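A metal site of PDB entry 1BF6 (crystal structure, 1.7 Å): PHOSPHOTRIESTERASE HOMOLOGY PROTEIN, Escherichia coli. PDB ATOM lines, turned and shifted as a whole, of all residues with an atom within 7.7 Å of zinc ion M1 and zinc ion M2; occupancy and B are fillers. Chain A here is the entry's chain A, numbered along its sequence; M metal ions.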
ATOM      1  N   HIS A  11     -31.205 -10.539  30.510  1.00  0.00           N
ATOM      2  CA  HIS A  11     -30.915  -9.097  30.400  1.00  0.00           C
ATOM      3  C   HIS A  11     -31.419  -8.516  29.095  1.00  0.00           C
ATOM      4  O   HIS A  11     -30.749  -8.598  28.075  1.00  0.00           O
ATOM      5  CB  HIS A  11     -29.410  -8.879  30.483  1.00  0.00           C
ATOM      6  CG  HIS A  11     -29.010  -7.434  30.575  1.00  0.00           C
ATOM      7  ND1 HIS A  11     -28.362  -6.895  31.676  1.00  0.00           N
ATOM      8  CD2 HIS A  11     -29.199  -6.418  29.707  1.00  0.00           C
ATOM      9  CE1 HIS A  11     -28.176  -5.595  31.446  1.00  0.00           C
ATOM     10  NE2 HIS A  11     -28.661  -5.253  30.270  1.00  0.00           N
ATOM     11  N   GLU A  12     -32.579  -7.883  29.155  1.00  0.00           N
ATOM     12  CA  GLU A  12     -33.197  -7.298  27.982  1.00  0.00           C
ATOM     13  C   GLU A  12     -33.872  -5.965  28.276  1.00  0.00           C
ATOM     14  O   GLU A  12     -34.058  -5.575  29.439  1.00  0.00           O
ATOM     15  CB  GLU A  12     -34.276  -8.232  27.427  1.00  0.00           C
ATOM     16  CG  GLU A  12     -33.783  -9.602  26.989  1.00  0.00           C
ATOM     17  CD  GLU A  12     -32.744  -9.529  25.904  1.00  0.00           C
ATOM     18  OE1 GLU A  12     -32.713  -8.544  25.135  1.00  0.00           O
ATOM     19  OE2 GLU A  12     -31.926 -10.468  25.822  1.00  0.00           O
ATOM     20  N   HIS A  13     -34.244  -5.267  27.210  1.00  0.00           N
ATOM     21  CA  HIS A  13     -34.976  -4.030  27.309  1.00  0.00           C
ATOM     22  C   HIS A  13     -36.167  -4.173  26.386  1.00  0.00           C
ATOM     23  O   HIS A  13     -35.978  -4.582  25.235  1.00  0.00           O
ATOM     24  CB  HIS A  13     -34.127  -2.845  26.856  1.00  0.00           C
ATOM     25  CG  HIS A  13     -32.959  -2.593  27.739  1.00  0.00           C
ATOM     26  ND1 HIS A  13     -33.034  -1.917  28.936  1.00  0.00           N
ATOM     27  CD2 HIS A  13     -31.681  -3.018  27.633  1.00  0.00           C
ATOM     28  CE1 HIS A  13     -31.835  -1.968  29.508  1.00  0.00           C
ATOM     29  NE2 HIS A  13     -30.988  -2.625  28.748  1.00  0.00           N
ATOM     30  N   ILE A  16     -37.136   1.122  26.509  1.00  0.00           N
ATOM     31  CA  ILE A  16     -36.041   1.943  26.991  1.00  0.00           C
ATOM     32  C   ILE A  16     -35.978   3.166  26.103  1.00  0.00           C
ATOM     33  O   ILE A  16     -36.300   3.092  24.908  1.00  0.00           O
ATOM     34  CB  ILE A  16     -34.688   1.178  26.988  1.00  0.00           C
ATOM     35  CG1 ILE A  16     -33.570   2.082  27.500  1.00  0.00           C
ATOM     36  CG2 ILE A  16     -34.370   0.634  25.584  1.00  0.00           C
ATOM     37  CD1 ILE A  16     -32.247   1.387  27.714  1.00  0.00           C
ATOM     38  N   GLU A  52     -36.302  -7.518  32.480  1.00  0.00           N
ATOM     39  CA  GLU A  52     -36.175  -6.190  31.911  1.00  0.00           C
ATOM     40  C   GLU A  52     -35.257  -5.293  32.764  1.00  0.00           C
ATOM     41  O   GLU A  52     -35.518  -5.055  33.950  1.00  0.00           O
ATOM     42  CB  GLU A  52     -37.572  -5.610  31.723  1.00  0.00           C
ATOM     43  CG  GLU A  52     -37.753  -4.859  30.406  1.00  0.00           C
ATOM     44  CD  GLU A  52     -37.300  -3.419  30.486  1.00  0.00           C
ATOM     45  OE1 GLU A  52     -37.062  -2.925  31.600  1.00  0.00           O
ATOM     46  OE2 GLU A  52     -37.196  -2.760  29.418  1.00  0.00           O
ATOM     47  N   MET A  53     -34.206  -4.769  32.121  1.00  0.00           N
ATOM     48  CA  MET A  53     -33.162  -3.974  32.748  1.00  0.00           C
ATOM     49  C   MET A  53     -33.256  -2.446  32.700  1.00  0.00           C
ATOM     50  O   MET A  53     -32.279  -1.760  33.023  1.00  0.00           O
ATOM     51  CB  MET A  53     -31.821  -4.364  32.130  1.00  0.00           C
ATOM     52  CG  MET A  53     -31.489  -5.851  32.246  1.00  0.00           C
ATOM     53  SD  MET A  53     -30.913  -6.318  33.909  1.00  0.00           S
ATOM     54  CE  MET A  53     -32.331  -7.042  34.503  1.00  0.00           C
ATOM     55  N   THR A  54     -34.405  -1.921  32.287  1.00  0.00           N
ATOM     56  CA  THR A  54     -34.594  -0.483  32.170  1.00  0.00           C
ATOM     57  C   THR A  54     -35.087   0.111  33.495  1.00  0.00           C
ATOM     58  O   THR A  54     -36.228  -0.102  33.855  1.00  0.00           O
ATOM     59  CB  THR A  54     -35.658  -0.120  31.081  1.00  0.00           C
ATOM     60  OG1 THR A  54     -35.356  -0.799  29.851  1.00  0.00           O
ATOM     61  CG2 THR A  54     -35.687   1.383  30.812  1.00  0.00           C
ATOM     62  N   MET A  58     -33.883   5.561  32.751  1.00  0.00           N
ATOM     63  CA  MET A  58     -33.380   5.002  31.509  1.00  0.00           C
ATOM     64  C   MET A  58     -34.572   5.000  30.550  1.00  0.00           C
ATOM     65  O   MET A  58     -34.456   4.623  29.383  1.00  0.00           O
ATOM     66  CB  MET A  58     -32.876   3.562  31.716  1.00  0.00           C
ATOM     67  CG  MET A  58     -31.489   3.454  32.324  1.00  0.00           C
ATOM     68  SD  MET A  58     -31.087   1.774  32.841  1.00  0.00           S
ATOM     69  CE  MET A  58     -30.556   1.048  31.243  1.00  0.00           C
ATOM     70  N   TYR A  83     -28.565   3.813  36.574  1.00  0.00           N
ATOM     71  CA  TYR A  83     -27.671   3.326  35.513  1.00  0.00           C
ATOM     72  C   TYR A  83     -26.160   3.468  35.676  1.00  0.00           C
ATOM     73  O   TYR A  83     -25.501   2.538  36.132  1.00  0.00           O
ATOM     74  CB  TYR A  83     -28.172   3.911  34.194  1.00  0.00           C
ATOM     75  CG  TYR A  83     -27.613   3.262  32.944  1.00  0.00           C
ATOM     76  CD1 TYR A  83     -27.154   1.948  32.940  1.00  0.00           C
ATOM     77  CD2 TYR A  83     -27.545   3.983  31.749  1.00  0.00           C
ATOM     78  CE1 TYR A  83     -26.640   1.367  31.792  1.00  0.00           C
ATOM     79  CE2 TYR A  83     -27.033   3.426  30.598  1.00  0.00           C
ATOM     80  CZ  TYR A  83     -26.585   2.122  30.623  1.00  0.00           C
ATOM     81  OH  TYR A  83     -26.040   1.601  29.472  1.00  0.00           O
ATOM     82  N   GLN A  84     -25.583   4.548  35.171  1.00  0.00           N
ATOM     83  CA  GLN A  84     -24.148   4.793  35.289  1.00  0.00           C
ATOM     84  C   GLN A  84     -23.915   6.291  35.335  1.00  0.00           C
ATOM     85  O   GLN A  84     -24.825   7.079  35.045  1.00  0.00           O
ATOM     86  CB  GLN A  84     -23.332   4.140  34.168  1.00  0.00           C
ATOM     87  CG  GLN A  84     -23.801   4.468  32.778  1.00  0.00           C
ATOM     88  CD  GLN A  84     -22.865   3.926  31.736  1.00  0.00           C
ATOM     89  OE1 GLN A  84     -21.675   4.214  31.737  1.00  0.00           O
ATOM     90  NE2 GLN A  84     -23.405   3.119  30.822  1.00  0.00           N
ATOM     91  N   GLU A 124     -30.506  -2.255  35.989  1.00  0.00           N
ATOM     92  CA  GLU A 124     -29.170  -2.565  35.742  1.00  0.00           C
ATOM     93  C   GLU A 124     -28.240  -1.550  36.408  1.00  0.00           C
ATOM     94  O   GLU A 124     -28.405  -0.376  36.038  1.00  0.00           O
ATOM     95  CB  GLU A 124     -28.623  -2.931  34.337  1.00  0.00           C
ATOM     96  CG  GLU A 124     -28.825  -1.797  33.307  1.00  0.00           C
ATOM     97  CD  GLU A 124     -28.213  -2.328  31.961  1.00  0.00           C
ATOM     98  OE1 GLU A 124     -27.063  -2.515  32.256  1.00  0.00           O
ATOM     99  OE2 GLU A 124     -29.164  -2.247  31.219  1.00  0.00           O
ATOM    100  N   ILE A 125     -27.535  -1.916  37.471  1.00  0.00           N
ATOM    101  CA  ILE A 125     -26.691  -0.944  38.131  1.00  0.00           C
ATOM    102  C   ILE A 125     -25.296  -1.046  37.573  1.00  0.00           C
ATOM    103  O   ILE A 125     -24.639  -2.082  37.650  1.00  0.00           O
ATOM    104  CB  ILE A 125     -26.793  -1.031  39.688  1.00  0.00           C
ATOM    105  CG1 ILE A 125     -26.289  -2.369  40.206  1.00  0.00           C
ATOM    106  CG2 ILE A 125     -28.283  -0.886  40.109  1.00  0.00           C
ATOM    107  CD1 ILE A 125     -26.216  -2.418  41.742  1.00  0.00           C
ATOM    108  N   GLY A 126     -24.868   0.034  36.925  1.00  0.00           N
ATOM    109  CA  GLY A 126     -23.563   0.015  36.299  1.00  0.00           C
ATOM    110  C   GLY A 126     -22.437   0.896  36.778  1.00  0.00           C
ATOM    111  O   GLY A 126     -22.586   1.781  37.635  1.00  0.00           O
ATOM    112  N   THR A 156     -25.989  -6.301  37.501  1.00  0.00           N
ATOM    113  CA  THR A 156     -25.157  -5.178  37.097  1.00  0.00           C
ATOM    114  C   THR A 156     -24.851  -4.961  35.605  1.00  0.00           C
ATOM    115  O   THR A 156     -25.156  -5.800  34.757  1.00  0.00           O
ATOM    116  CB  THR A 156     -23.802  -5.229  37.836  1.00  0.00           C
ATOM    117  OG1 THR A 156     -22.918  -6.131  37.148  1.00  0.00           O
ATOM    118  CG2 THR A 156     -23.977  -5.705  39.299  1.00  0.00           C
ATOM    119  N   HIS A 157     -24.221  -3.819  35.318  1.00  0.00           N
ATOM    120  CA  HIS A 157     -23.762  -3.424  33.979  1.00  0.00           C
ATOM    121  C   HIS A 157     -22.269  -3.165  34.098  1.00  0.00           C
ATOM    122  O   HIS A 157     -21.851  -2.324  34.905  1.00  0.00           O
ATOM    123  CB  HIS A 157     -24.428  -2.110  33.495  1.00  0.00           C
ATOM    124  CG  HIS A 157     -23.696  -1.406  32.379  1.00  0.00           C
ATOM    125  ND1 HIS A 157     -24.223  -1.330  31.107  1.00  0.00           N
ATOM    126  CD2 HIS A 157     -22.548  -0.681  32.415  1.00  0.00           C
ATOM    127  CE1 HIS A 157     -23.395  -0.573  30.407  1.00  0.00           C
ATOM    128  NE2 HIS A 157     -22.366  -0.154  31.164  1.00  0.00           N
ATOM    129  N   THR A 158     -21.450  -3.924  33.376  1.00  0.00           N
ATOM    130  CA  THR A 158     -20.026  -3.640  33.366  1.00  0.00           C
ATOM    131  C   THR A 158     -19.812  -3.008  31.983  1.00  0.00           C
ATOM    132  O   THR A 158     -20.402  -3.457  30.988  1.00  0.00           O
ATOM    133  CB  THR A 158     -19.087  -4.880  33.526  1.00  0.00           C
ATOM    134  OG1 THR A 158     -19.314  -5.829  32.471  1.00  0.00           O
ATOM    135  CG2 THR A 158     -19.265  -5.535  34.898  1.00  0.00           C
ATOM    136  N   SER A 159     -19.071  -1.903  31.955  1.00  0.00           N
ATOM    137  CA  SER A 159     -18.780  -1.204  30.714  1.00  0.00           C
ATOM    138  C   SER A 159     -17.625  -1.905  30.010  1.00  0.00           C
ATOM    139  O   SER A 159     -16.494  -1.910  30.488  1.00  0.00           O
ATOM    140  CB  SER A 159     -18.462   0.265  30.993  1.00  0.00           C
ATOM    141  OG  SER A 159     -19.655   0.976  31.240  1.00  0.00           O
ATOM    142  N   GLY A 184     -23.380  -8.329  34.703  1.00  0.00           N
ATOM    143  CA  GLY A 184     -23.738  -8.152  33.304  1.00  0.00           C
ATOM    144  C   GLY A 184     -22.595  -7.799  32.362  1.00  0.00           C
ATOM    145  O   GLY A 184     -21.590  -7.216  32.780  1.00  0.00           O
ATOM    146  N   HIS A 185     -22.760  -8.171  31.091  1.00  0.00           N
ATOM    147  CA  HIS A 185     -21.778  -7.907  30.036  1.00  0.00           C
ATOM    148  C   HIS A 185     -20.370  -8.404  30.267  1.00  0.00           C
ATOM    149  O   HIS A 185     -19.408  -7.657  30.090  1.00  0.00           O
ATOM    150  CB  HIS A 185     -21.720  -6.413  29.732  1.00  0.00           C
ATOM    151  CG  HIS A 185     -23.040  -5.733  29.760  1.00  0.00           C
ATOM    152  ND1 HIS A 185     -24.213  -6.299  29.295  1.00  0.00           N
ATOM    153  CD2 HIS A 185     -23.388  -4.535  30.281  1.00  0.00           C
ATOM    154  CE1 HIS A 185     -25.194  -5.456  29.558  1.00  0.00           C
ATOM    155  NE2 HIS A 185     -24.713  -4.388  30.147  1.00  0.00           N
ATOM    156  N   ASP A 208     -24.451 -11.675  27.911  1.00  0.00           N
ATOM    157  CA  ASP A 208     -25.691 -11.021  27.463  1.00  0.00           C
ATOM    158  C   ASP A 208     -25.592 -10.035  26.295  1.00  0.00           C
ATOM    159  O   ASP A 208     -26.513  -9.249  26.077  1.00  0.00           O
ATOM    160  CB  ASP A 208     -26.366 -10.304  28.643  1.00  0.00           C
ATOM    161  CG  ASP A 208     -25.418  -9.389  29.403  1.00  0.00           C
ATOM    162  OD1 ASP A 208     -24.442  -8.884  28.798  1.00  0.00           O
ATOM    163  OD2 ASP A 208     -25.620  -9.216  30.625  1.00  0.00           O
ATOM    164  N   THR A 209     -24.463 -10.047  25.580  1.00  0.00           N
ATOM    165  CA  THR A 209     -24.286  -9.171  24.427  1.00  0.00           C
ATOM    166  C   THR A 209     -24.186 -10.031  23.151  1.00  0.00           C
ATOM    167  O   THR A 209     -23.552  -9.637  22.153  1.00  0.00           O
ATOM    168  CB  THR A 209     -23.057  -8.250  24.575  1.00  0.00           C
ATOM    169  OG1 THR A 209     -21.862  -9.032  24.742  1.00  0.00           O
ATOM    170  CG2 THR A 209     -23.216  -7.308  25.783  1.00  0.00           C
ATOM    171  N   LYS A 212     -23.828  -8.965  19.238  1.00  0.00           N
ATOM    172  CA  LYS A 212     -23.147  -7.677  19.082  1.00  0.00           C
ATOM    173  C   LYS A 212     -21.703  -7.930  18.656  1.00  0.00           C
ATOM    174  O   LYS A 212     -20.740  -7.584  19.331  1.00  0.00           O
ATOM    175  CB  LYS A 212     -23.229  -6.873  20.402  1.00  0.00           C
ATOM    176  CG  LYS A 212     -24.687  -6.662  20.830  1.00  0.00           C
ATOM    177  CD  LYS A 212     -24.909  -5.612  21.907  1.00  0.00           C
ATOM    178  CE  LYS A 212     -26.403  -5.417  22.102  1.00  0.00           C
ATOM    179  NZ  LYS A 212     -26.711  -4.286  23.008  1.00  0.00           N
ATOM    180  N   MET A 241     -29.393 -11.109  24.976  1.00  0.00           N
ATOM    181  CA  MET A 241     -29.032 -10.302  23.796  1.00  0.00           C
ATOM    182  C   MET A 241     -28.814  -8.820  24.130  1.00  0.00           C
ATOM    183  O   MET A 241     -28.137  -8.090  23.385  1.00  0.00           O
ATOM    184  CB  MET A 241     -30.166 -10.385  22.764  1.00  0.00           C
ATOM    185  CG  MET A 241     -30.587 -11.786  22.323  1.00  0.00           C
ATOM    186  SD  MET A 241     -29.270 -12.602  21.480  1.00  0.00           S
ATOM    187  CE  MET A 241     -29.198 -11.610  19.997  1.00  0.00           C
ATOM    188  N   ASP A 242     -29.417  -8.373  25.223  1.00  0.00           N
ATOM    189  CA  ASP A 242     -29.374  -6.968  25.636  1.00  0.00           C
ATOM    190  C   ASP A 242     -29.831  -6.053  24.480  1.00  0.00           C
ATOM    191  O   ASP A 242     -29.100  -5.137  24.076  1.00  0.00           O
ATOM    192  CB  ASP A 242     -27.964  -6.554  26.096  1.00  0.00           C
ATOM    193  CG  ASP A 242     -27.928  -5.155  26.699  1.00  0.00           C
ATOM    194  OD1 ASP A 242     -29.004  -4.640  27.091  1.00  0.00           O
ATOM    195  OD2 ASP A 242     -26.836  -4.584  26.770  1.00  0.00           O
ATOM    196  N   ILE A 243     -31.018  -6.346  23.925  1.00  0.00           N
ATOM    197  CA  ILE A 243     -31.594  -5.532  22.847  1.00  0.00           C
ATOM    198  C   ILE A 243     -31.854  -4.134  23.431  1.00  0.00           C
ATOM    199  O   ILE A 243     -32.422  -4.002  24.521  1.00  0.00           O
ATOM    200  CB  ILE A 243     -32.932  -6.141  22.323  1.00  0.00           C
ATOM    201  CG1 ILE A 243     -32.680  -7.499  21.658  1.00  0.00           C
ATOM    202  CG2 ILE A 243     -33.617  -5.185  21.364  1.00  0.00           C
ATOM    203  CD1 ILE A 243     -31.684  -7.458  20.513  1.00  0.00           C
ATOM    204  N   THR A 244     -31.421  -3.108  22.698  1.00  0.00           N
ATOM    205  CA  THR A 244     -31.549  -1.724  23.144  1.00  0.00           C
ATOM    206  C   THR A 244     -31.998  -0.718  22.062  1.00  0.00           C
ATOM    207  O   THR A 244     -32.386   0.402  22.387  1.00  0.00           O
ATOM    208  CB  THR A 244     -30.195  -1.192  23.677  1.00  0.00           C
ATOM    209  OG1 THR A 244     -29.201  -1.266  22.647  1.00  0.00           O
ATOM    210  CG2 THR A 244     -29.696  -1.990  24.889  1.00  0.00           C
HETATM  211 ZN    ZN M   1     -25.955  -2.612  30.372  1.00  0.00          ZN
HETATM  212 ZN    ZN M   2     -28.973  -3.319  29.110  1.00  0.00          ZN
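Four residues have an atom within 4 Å of zinc ion M2: His 11, His 13, Glu 124 and Asp 242.
The nearest printed residue that does not touch zinc ion M2 is Met 53 (4.3 Å).
Zinc ion M1 is bound by NE2 of His 185, OE1 of Glu 124 and ND1 of His 157.
Zinc ion M1 has three donor atoms within binding distance.
N of His 13 lies close to O of Ile 243, 3.5 Å away.
O of His 185 lies within hydrogen-bond range of OG1 of Thr 158.
The backbone NH of Glu 124 sits close to the backbone carbonyl oxygen of Met 53 (3.5 Å).
A ring nitrogen (NE2) of His 157 sits at hydrogen-bond distance from the side-chain amide nitrogen of Gln 84.
NE2 of His 157 sits at hydrogen-bond distance from OG of Ser 159, 2.9 Å away.
A ring nitrogen (ND1) of His 11 sits close to the side-chain sulfur (SD) of Met 53 (3.4 Å).
The side-chain carboxylate of Glu 12 is in hydrogen-bond range of the backbone NH of Asp 242, 3.3 Å away.
The side-chain carboxylate of Asp 242 lies within salt-bridge range of the side-chain amino group of Lys 212, at 3.8 Å.
Zinc ion M2 is bound by a ring nitrogen (NE2) of His 13, a ring nitrogen (NE2) of His 11, the side-chain carboxylate of Glu 124 and the side-chain carboxylate of Asp 242.
Zinc ion M2 has four donor atoms within binding distance.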
